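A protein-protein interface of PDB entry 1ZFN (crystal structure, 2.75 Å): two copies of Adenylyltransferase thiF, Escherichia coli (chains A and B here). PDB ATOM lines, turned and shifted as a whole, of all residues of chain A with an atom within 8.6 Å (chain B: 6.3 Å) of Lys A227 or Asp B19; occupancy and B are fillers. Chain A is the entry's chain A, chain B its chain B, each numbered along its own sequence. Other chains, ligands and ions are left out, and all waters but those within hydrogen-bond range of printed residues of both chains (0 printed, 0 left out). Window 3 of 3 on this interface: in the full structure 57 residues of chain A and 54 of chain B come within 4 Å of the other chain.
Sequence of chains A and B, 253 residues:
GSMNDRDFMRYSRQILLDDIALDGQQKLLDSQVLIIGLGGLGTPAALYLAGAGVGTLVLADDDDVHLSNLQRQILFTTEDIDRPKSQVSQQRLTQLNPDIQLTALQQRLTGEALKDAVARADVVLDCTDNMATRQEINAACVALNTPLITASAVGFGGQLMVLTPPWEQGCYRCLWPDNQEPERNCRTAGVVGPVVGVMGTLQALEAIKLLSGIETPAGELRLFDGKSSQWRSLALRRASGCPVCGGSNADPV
The side-chain amino group (NZ) of Lys A227 is in salt-bridge range of the side-chain carboxylate (OD2) of Asp B19, 3.5 Å away.
NZ of Lys B209 lies within hydrogen-bond range of OG of Ser A229, at 2.7 Å.
O of Gly A226 sits at hydrogen-bond distance from NZ of Lys B209, 2.7 Å away.
The backbone carbonyl oxygen of Lys A227 lies within hydrogen-bond range of the side-chain amino group of Lys B209.
O of Ser A228 lies within hydrogen-bond range of NE2 of Gln A230, at 3.3 Å.
The side-chain hydroxyl (OG1) of Thr B216 sits close to the side-chain amino group (NZ) of Lys B209 (3.3 Å).
The backbone carbonyl oxygen (O) of Phe A156 sits at hydrogen-bond distance from the backbone NH (N) of Gly A226 (2.7 Å).
The side-chain carboxylate of Asp A225 sits at hydrogen-bond distance from the side-chain hydroxyl of Ser A228 (2.9 Å).
O of Gly A155 sits at hydrogen-bond distance from N of Val A192 (2.8 Å).
The backbone carbonyl oxygen of Lys B209 lies within hydrogen-bond range of the backbone NH of Ile B214 (2.6 Å).
Gly A155 touches Leu B17 (CA to CD2, 3.8 Å).
Phe A156 touches Asp B19 (CE1 to CB, 3.7 Å).
CZ of Phe A156 touches CD1 of Ile B214 (3.4 Å).
Leu B17 touches Arg A187 (CD2 to O, 3.9 Å).
Val A192 touches Leu B17 (CG2 to CD1, 3.6 Å).
Val A195 touches Leu B205 (CG2 to CD1, 3.9 Å).
Phe A224 touches Leu B205.
O of Gly A226 touches CD2 of Leu B205, at 3.8 Å.
Lys A227 touches Ile B214 (CD to CG2, 3.8 Å).
OG1 of Thr B216 touches O of Lys A227, 3.7 Å away.
Of chain B, only Asp B19, Lys B209, Ile B214, Glu B215 and Thr B216 come within 4 Å of Lys A227.
Of the printed residues of chain B, Gly A155 touches Leu B17 (3.8 Å).
Printed residues of chain B within 4 Å of Val A192: Leu B17 and Leu B205.
Of the printed residues of chain B, Val A195 touches Leu B205 (3.9 Å).
Of the printed residues of chain A, Lys B209 touches Gly A226, Lys A227 and Ser A229.
Gly B213 touches none of the printed residues of chain A.
Gly A157 touches none of the printed residues of chain B.
The nearest residue of chain A that does not touch Asp B19 is Arg A187 (6.7 Å).
Hydrophobic or aromatic side chains of chain A that line the printed part of chain B: Phe A156, Val A192, Val A195 and Phe A224.
Hydrophobic or aromatic side chains of chain B that line the printed part of chain A: Leu B17, Leu B205, Ile B214 and Pro B217.
No position is printed for both chains.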
ATOM      1  N   VAL A 154      -2.348 -16.295  25.830  1.00  0.00           N
ATOM      2  CA  VAL A 154      -2.993 -17.603  25.966  1.00  0.00           C
ATOM      3  C   VAL A 154      -1.910 -18.677  25.999  1.00  0.00           C
ATOM      4  O   VAL A 154      -1.107 -18.797  25.072  1.00  0.00           O
ATOM      5  CB  VAL A 154      -3.929 -17.914  24.772  1.00  0.00           C
ATOM      6  CG1 VAL A 154      -4.806 -19.088  25.116  1.00  0.00           C
ATOM      7  CG2 VAL A 154      -4.779 -16.707  24.429  1.00  0.00           C
ATOM      8  N   GLY A 155      -1.893 -19.457  27.068  1.00  0.00           N
ATOM      9  CA  GLY A 155      -0.891 -20.492  27.186  1.00  0.00           C
ATOM     10  C   GLY A 155       0.516 -19.932  27.221  1.00  0.00           C
ATOM     11  O   GLY A 155       0.922 -19.314  28.217  1.00  0.00           O
ATOM     12  N   PHE A 156       1.260 -20.150  26.139  1.00  0.00           N
ATOM     13  CA  PHE A 156       2.639 -19.685  26.032  1.00  0.00           C
ATOM     14  C   PHE A 156       2.762 -18.591  24.995  1.00  0.00           C
ATOM     15  O   PHE A 156       3.873 -18.197  24.644  1.00  0.00           O
ATOM     16  CB  PHE A 156       3.581 -20.809  25.598  1.00  0.00           C
ATOM     17  CG  PHE A 156       4.035 -21.702  26.709  1.00  0.00           C
ATOM     18  CD1 PHE A 156       3.275 -22.805  27.095  1.00  0.00           C
ATOM     19  CD2 PHE A 156       5.246 -21.457  27.359  1.00  0.00           C
ATOM     20  CE1 PHE A 156       3.722 -23.654  28.116  1.00  0.00           C
ATOM     21  CE2 PHE A 156       5.699 -22.293  28.374  1.00  0.00           C
ATOM     22  CZ  PHE A 156       4.938 -23.395  28.755  1.00  0.00           C
ATOM     23  N   GLY A 157       1.640 -18.105  24.487  1.00  0.00           N
ATOM     24  CA  GLY A 157       1.729 -17.087  23.461  1.00  0.00           C
ATOM     25  C   GLY A 157       1.135 -15.754  23.841  1.00  0.00           C
ATOM     26  O   GLY A 157       0.107 -15.685  24.530  1.00  0.00           O
ATOM     27  N   GLY A 158       1.791 -14.690  23.391  1.00  0.00           N
ATOM     28  CA  GLY A 158       1.326 -13.352  23.687  1.00  0.00           C
ATOM     29  C   GLY A 158       1.231 -12.519  22.427  1.00  0.00           C
ATOM     30  O   GLY A 158       1.952 -12.752  21.446  1.00  0.00           O
ATOM     31  N   ARG A 187      -6.186 -24.167  23.349  1.00  0.00           N
ATOM     32  CA  ARG A 187      -5.061 -23.943  24.255  1.00  0.00           C
ATOM     33  C   ARG A 187      -5.479 -23.277  25.558  1.00  0.00           C
ATOM     34  O   ARG A 187      -4.883 -23.527  26.605  1.00  0.00           O
ATOM     35  CB  ARG A 187      -4.007 -23.041  23.605  1.00  0.00           C
ATOM     36  CG  ARG A 187      -3.125 -23.671  22.550  1.00  0.00           C
ATOM     37  CD  ARG A 187      -1.987 -22.708  22.229  1.00  0.00           C
ATOM     38  NE  ARG A 187      -0.979 -23.284  21.344  1.00  0.00           N
ATOM     39  CZ  ARG A 187       0.208 -22.731  21.110  1.00  0.00           C
ATOM     40  NH1 ARG A 187       0.538 -21.588  21.699  1.00  0.00           N
ATOM     41  NH2 ARG A 187       1.067 -23.322  20.291  1.00  0.00           N
ATOM     42  N   VAL A 192       0.643 -19.049  30.961  1.00  0.00           N
ATOM     43  CA  VAL A 192       1.917 -18.987  31.694  1.00  0.00           C
ATOM     44  C   VAL A 192       2.153 -17.584  32.267  1.00  0.00           C
ATOM     45  O   VAL A 192       2.155 -16.596  31.523  1.00  0.00           O
ATOM     46  CB  VAL A 192       3.105 -19.325  30.775  1.00  0.00           C
ATOM     47  CG1 VAL A 192       4.409 -19.222  31.547  1.00  0.00           C
ATOM     48  CG2 VAL A 192       2.932 -20.709  30.193  1.00  0.00           C
ATOM     49  N   VAL A 195       4.695 -15.187  30.649  1.00  0.00           N
ATOM     50  CA  VAL A 195       4.280 -14.839  29.297  1.00  0.00           C
ATOM     51  C   VAL A 195       3.301 -13.662  29.298  1.00  0.00           C
ATOM     52  O   VAL A 195       3.531 -12.665  28.618  1.00  0.00           O
ATOM     53  CB  VAL A 195       3.648 -16.042  28.576  1.00  0.00           C
ATOM     54  CG1 VAL A 195       3.122 -15.619  27.217  1.00  0.00           C
ATOM     55  CG2 VAL A 195       4.693 -17.131  28.407  1.00  0.00           C
ATOM     56  N   PHE A 224       4.771 -13.067  20.511  1.00  0.00           N
ATOM     57  CA  PHE A 224       5.803 -13.659  21.342  1.00  0.00           C
ATOM     58  C   PHE A 224       5.507 -15.139  21.565  1.00  0.00           C
ATOM     59  O   PHE A 224       4.393 -15.528  21.903  1.00  0.00           O
ATOM     60  CB  PHE A 224       5.885 -12.949  22.706  1.00  0.00           C
ATOM     61  CG  PHE A 224       6.836 -13.604  23.682  1.00  0.00           C
ATOM     62  CD1 PHE A 224       8.146 -13.918  23.301  1.00  0.00           C
ATOM     63  CD2 PHE A 224       6.433 -13.886  24.983  1.00  0.00           C
ATOM     64  CE1 PHE A 224       9.049 -14.504  24.204  1.00  0.00           C
ATOM     65  CE2 PHE A 224       7.324 -14.473  25.907  1.00  0.00           C
ATOM     66  CZ  PHE A 224       8.641 -14.783  25.515  1.00  0.00           C
ATOM     67  N   ASP A 225       6.517 -15.967  21.368  1.00  0.00           N
ATOM     68  CA  ASP A 225       6.356 -17.382  21.600  1.00  0.00           C
ATOM     69  C   ASP A 225       7.161 -17.733  22.849  1.00  0.00           C
ATOM     70  O   ASP A 225       8.384 -17.818  22.802  1.00  0.00           O
ATOM     71  CB  ASP A 225       6.863 -18.188  20.404  1.00  0.00           C
ATOM     72  CG  ASP A 225       6.685 -19.681  20.593  1.00  0.00           C
ATOM     73  OD1 ASP A 225       7.242 -20.431  19.769  1.00  0.00           O
ATOM     74  OD2 ASP A 225       5.993 -20.101  21.551  1.00  0.00           O
ATOM     75  N   GLY A 226       6.457 -17.936  23.958  1.00  0.00           N
ATOM     76  CA  GLY A 226       7.109 -18.260  25.208  1.00  0.00           C
ATOM     77  C   GLY A 226       7.750 -19.625  25.207  1.00  0.00           C
ATOM     78  O   GLY A 226       8.681 -19.877  25.974  1.00  0.00           O
ATOM     79  N   LYS A 227       7.250 -20.514  24.356  1.00  0.00           N
ATOM     80  CA  LYS A 227       7.790 -21.862  24.264  1.00  0.00           C
ATOM     81  C   LYS A 227       9.177 -21.831  23.658  1.00  0.00           C
ATOM     82  O   LYS A 227      10.090 -22.474  24.163  1.00  0.00           O
ATOM     83  CB  LYS A 227       6.887 -22.738  23.403  1.00  0.00           C
ATOM     84  CG  LYS A 227       5.776 -23.421  24.161  1.00  0.00           C
ATOM     85  CD  LYS A 227       6.290 -24.640  24.891  1.00  0.00           C
ATOM     86  CE  LYS A 227       6.703 -25.718  23.907  1.00  0.00           C
ATOM     87  NZ  LYS A 227       5.585 -26.063  22.984  1.00  0.00           N
ATOM     88  N   SER A 228       9.343 -21.087  22.569  1.00  0.00           N
ATOM     89  CA  SER A 228      10.651 -21.017  21.922  1.00  0.00           C
ATOM     90  C   SER A 228      11.389 -19.742  22.286  1.00  0.00           C
ATOM     91  O   SER A 228      12.566 -19.590  21.971  1.00  0.00           O
ATOM     92  CB  SER A 228      10.511 -21.088  20.398  1.00  0.00           C
ATOM     93  OG  SER A 228      10.072 -19.852  19.858  1.00  0.00           O
ATOM     94  N   SER A 229      10.687 -18.828  22.944  1.00  0.00           N
ATOM     95  CA  SER A 229      11.266 -17.556  23.342  1.00  0.00           C
ATOM     96  C   SER A 229      11.655 -16.705  22.140  1.00  0.00           C
ATOM     97  O   SER A 229      12.684 -16.033  22.167  1.00  0.00           O
ATOM     98  CB  SER A 229      12.490 -17.780  24.228  1.00  0.00           C
ATOM     99  OG  SER A 229      12.103 -18.130  25.539  1.00  0.00           O
ATOM    100  N   GLN A 230      10.828 -16.728  21.096  1.00  0.00           N
ATOM    101  CA  GLN A 230      11.091 -15.951  19.887  1.00  0.00           C
ATOM    102  C   GLN A 230      10.013 -14.911  19.603  1.00  0.00           C
ATOM    103  O   GLN A 230       8.843 -15.117  19.928  1.00  0.00           O
ATOM    104  CB  GLN A 230      11.203 -16.881  18.689  1.00  0.00           C
ATOM    105  CG  GLN A 230      12.354 -17.842  18.777  1.00  0.00           C
ATOM    106  CD  GLN A 230      13.643 -17.145  19.135  1.00  0.00           C
ATOM    107  OE1 GLN A 230      13.872 -16.007  18.732  1.00  0.00           O
ATOM    108  NE2 GLN A 230      14.500 -17.826  19.891  1.00  0.00           N
ATOM    109  N   GLN B  14      -1.878 -23.245  35.015  1.00  0.00           N
ATOM    110  CA  GLN B  14      -0.638 -23.856  34.537  1.00  0.00           C
ATOM    111  C   GLN B  14      -0.917 -25.353  34.380  1.00  0.00           C
ATOM    112  O   GLN B  14      -0.581 -25.968  33.359  1.00  0.00           O
ATOM    113  CB  GLN B  14       0.491 -23.691  35.554  1.00  0.00           C
ATOM    114  CG  GLN B  14       0.901 -22.276  35.823  1.00  0.00           C
ATOM    115  CD  GLN B  14       2.042 -22.173  36.814  1.00  0.00           C
ATOM    116  OE1 GLN B  14       2.580 -21.088  37.026  1.00  0.00           O
ATOM    117  NE2 GLN B  14       2.415 -23.291  37.431  1.00  0.00           N
ATOM    118  N   LEU B  17      -2.156 -26.771  31.298  1.00  0.00           N
ATOM    119  CA  LEU B  17      -1.346 -26.548  30.104  1.00  0.00           C
ATOM    120  C   LEU B  17      -0.579 -27.810  29.803  1.00  0.00           C
ATOM    121  O   LEU B  17       0.086 -28.366  30.678  1.00  0.00           O
ATOM    122  CB  LEU B  17      -0.377 -25.372  30.302  1.00  0.00           C
ATOM    123  CG  LEU B  17      -1.009 -23.978  30.177  1.00  0.00           C
ATOM    124  CD1 LEU B  17       0.026 -22.893  30.459  1.00  0.00           C
ATOM    125  CD2 LEU B  17      -1.602 -23.828  28.776  1.00  0.00           C
ATOM    126  N   ASP B  18      -0.663 -28.257  28.559  1.00  0.00           N
ATOM    127  CA  ASP B  18      -0.002 -29.484  28.156  1.00  0.00           C
ATOM    128  C   ASP B  18       1.489 -29.541  28.439  1.00  0.00           C
ATOM    129  O   ASP B  18       2.007 -30.596  28.803  1.00  0.00           O
ATOM    130  CB  ASP B  18      -0.270 -29.759  26.679  1.00  0.00           C
ATOM    131  CG  ASP B  18      -1.727 -30.072  26.411  1.00  0.00           C
ATOM    132  OD1 ASP B  18      -2.262 -30.995  27.064  1.00  0.00           O
ATOM    133  OD2 ASP B  18      -2.338 -29.398  25.555  1.00  0.00           O
ATOM    134  N   ASP B  19       2.182 -28.418  28.290  1.00  0.00           N
ATOM    135  CA  ASP B  19       3.618 -28.400  28.536  1.00  0.00           C
ATOM    136  C   ASP B  19       4.031 -28.275  30.005  1.00  0.00           C
ATOM    137  O   ASP B  19       5.213 -28.381  30.324  1.00  0.00           O
ATOM    138  CB  ASP B  19       4.268 -27.311  27.696  1.00  0.00           C
ATOM    139  CG  ASP B  19       4.132 -27.577  26.216  1.00  0.00           C
ATOM    140  OD1 ASP B  19       4.762 -28.535  25.720  1.00  0.00           O
ATOM    141  OD2 ASP B  19       3.380 -26.833  25.554  1.00  0.00           O
ATOM    142  N   ILE B  20       3.071 -28.058  30.900  1.00  0.00           N
ATOM    143  CA  ILE B  20       3.395 -27.975  32.312  1.00  0.00           C
ATOM    144  C   ILE B  20       2.679 -29.126  32.997  1.00  0.00           C
ATOM    145  O   ILE B  20       3.310 -30.110  33.370  1.00  0.00           O
ATOM    146  CB  ILE B  20       2.949 -26.639  32.946  1.00  0.00           C
ATOM    147  CG1 ILE B  20       3.633 -25.459  32.256  1.00  0.00           C
ATOM    148  CG2 ILE B  20       3.373 -26.608  34.400  1.00  0.00           C
ATOM    149  CD1 ILE B  20       5.133 -25.496  32.383  1.00  0.00           C
ATOM    150  N   ALA B  21       1.365 -29.003  33.157  1.00  0.00           N
ATOM    151  CA  ALA B  21       0.561 -30.055  33.764  1.00  0.00           C
ATOM    152  C   ALA B  21       0.904 -30.378  35.203  1.00  0.00           C
ATOM    153  O   ALA B  21       1.694 -29.675  35.847  1.00  0.00           O
ATOM    154  CB  ALA B  21       0.641 -31.311  32.924  1.00  0.00           C
ATOM    155  N   GLY B  24       4.684 -30.949  35.670  1.00  0.00           N
ATOM    156  CA  GLY B  24       5.504 -29.749  35.773  1.00  0.00           C
ATOM    157  C   GLY B  24       5.294 -29.051  37.104  1.00  0.00           C
ATOM    158  O   GLY B  24       6.244 -28.647  37.770  1.00  0.00           O
ATOM    159  N   LEU B 205      10.485 -16.794  33.159  1.00  0.00           N
ATOM    160  CA  LEU B 205       9.957 -17.692  32.150  1.00  0.00           C
ATOM    161  C   LEU B 205      10.961 -18.798  31.870  1.00  0.00           C
ATOM    162  O   LEU B 205      10.591 -19.969  31.788  1.00  0.00           O
ATOM    163  CB  LEU B 205       9.656 -16.924  30.864  1.00  0.00           C
ATOM    164  CG  LEU B 205       9.243 -17.784  29.664  1.00  0.00           C
ATOM    165  CD1 LEU B 205       7.948 -18.467  30.003  1.00  0.00           C
ATOM    166  CD2 LEU B 205       9.091 -16.943  28.399  1.00  0.00           C
ATOM    167  N   LYS B 209      10.560 -22.834  32.526  1.00  0.00           N
ATOM    168  CA  LYS B 209      10.750 -23.746  31.402  1.00  0.00           C
ATOM    169  C   LYS B 209      11.873 -24.747  31.641  1.00  0.00           C
ATOM    170  O   LYS B 209      11.800 -25.896  31.191  1.00  0.00           O
ATOM    171  CB  LYS B 209      11.036 -22.958  30.122  1.00  0.00           C
ATOM    172  CG  LYS B 209       9.810 -22.228  29.573  1.00  0.00           C
ATOM    173  CD  LYS B 209      10.187 -21.098  28.638  1.00  0.00           C
ATOM    174  CE  LYS B 209      10.825 -21.627  27.388  1.00  0.00           C
ATOM    175  NZ  LYS B 209      11.211 -20.540  26.472  1.00  0.00           N
ATOM    176  N   SER B 212      10.758 -27.277  34.530  1.00  0.00           N
ATOM    177  CA  SER B 212       9.683 -28.168  34.111  1.00  0.00           C
ATOM    178  C   SER B 212      10.079 -28.991  32.877  1.00  0.00           C
ATOM    179  O   SER B 212       9.272 -29.732  32.321  1.00  0.00           O
ATOM    180  CB  SER B 212       8.413 -27.355  33.819  1.00  0.00           C
ATOM    181  OG  SER B 212       8.508 -26.685  32.576  1.00  0.00           O
ATOM    182  N   GLY B 213      11.323 -28.841  32.443  1.00  0.00           N
ATOM    183  CA  GLY B 213      11.812 -29.594  31.304  1.00  0.00           C
ATOM    184  C   GLY B 213      11.385 -29.177  29.908  1.00  0.00           C
ATOM    185  O   GLY B 213      11.434 -29.992  28.991  1.00  0.00           O
ATOM    186  N   ILE B 214      10.974 -27.928  29.720  1.00  0.00           N
ATOM    187  CA  ILE B 214      10.566 -27.482  28.390  1.00  0.00           C
ATOM    188  C   ILE B 214      11.811 -27.148  27.547  1.00  0.00           C
ATOM    189  O   ILE B 214      12.704 -26.435  27.998  1.00  0.00           O
ATOM    190  CB  ILE B 214       9.630 -26.250  28.484  1.00  0.00           C
ATOM    191  CG1 ILE B 214       8.417 -26.578  29.357  1.00  0.00           C
ATOM    192  CG2 ILE B 214       9.142 -25.855  27.103  1.00  0.00           C
ATOM    193  CD1 ILE B 214       7.545 -25.395  29.671  1.00  0.00           C
ATOM    194  N   GLU B 215      11.870 -27.691  26.333  1.00  0.00           N
ATOM    195  CA  GLU B 215      12.995 -27.470  25.419  1.00  0.00           C
ATOM    196  C   GLU B 215      13.043 -26.009  24.997  1.00  0.00           C
ATOM    197  O   GLU B 215      12.058 -25.483  24.480  1.00  0.00           O
ATOM    198  CB  GLU B 215      12.826 -28.327  24.166  1.00  0.00           C
ATOM    199  CG  GLU B 215      12.469 -29.771  24.433  1.00  0.00           C
ATOM    200  CD  GLU B 215      11.795 -30.417  23.240  1.00  0.00           C
ATOM    201  OE1 GLU B 215      10.702 -29.950  22.851  1.00  0.00           O
ATOM    202  OE2 GLU B 215      12.355 -31.388  22.689  1.00  0.00           O
ATOM    203  N   THR B 216      14.185 -25.355  25.197  1.00  0.00           N
ATOM    204  CA  THR B 216      14.318 -23.949  24.825  1.00  0.00           C
ATOM    205  C   THR B 216      15.736 -23.603  24.412  1.00  0.00           C
ATOM    206  O   THR B 216      16.690 -24.066  25.032  1.00  0.00           O
ATOM    207  CB  THR B 216      13.961 -23.024  25.995  1.00  0.00           C
ATOM    208  OG1 THR B 216      12.726 -23.449  26.575  1.00  0.00           O
ATOM    209  CG2 THR B 216      13.827 -21.580  25.514  1.00  0.00           C
ATOM    210  N   PRO B 217      15.891 -22.779  23.359  1.00  0.00           N
ATOM    211  CA  PRO B 217      17.216 -22.368  22.878  1.00  0.00           C
ATOM    212  C   PRO B 217      17.983 -21.747  24.042  1.00  0.00           C
ATOM    213  O   PRO B 217      17.402 -21.012  24.845  1.00  0.00           O
ATOM    214  CB  PRO B 217      16.882 -21.354  21.795  1.00  0.00           C
ATOM    215  CG  PRO B 217      15.609 -21.917  21.216  1.00  0.00           C
ATOM    216  CD  PRO B 217      14.831 -22.288  22.458  1.00  0.00           C
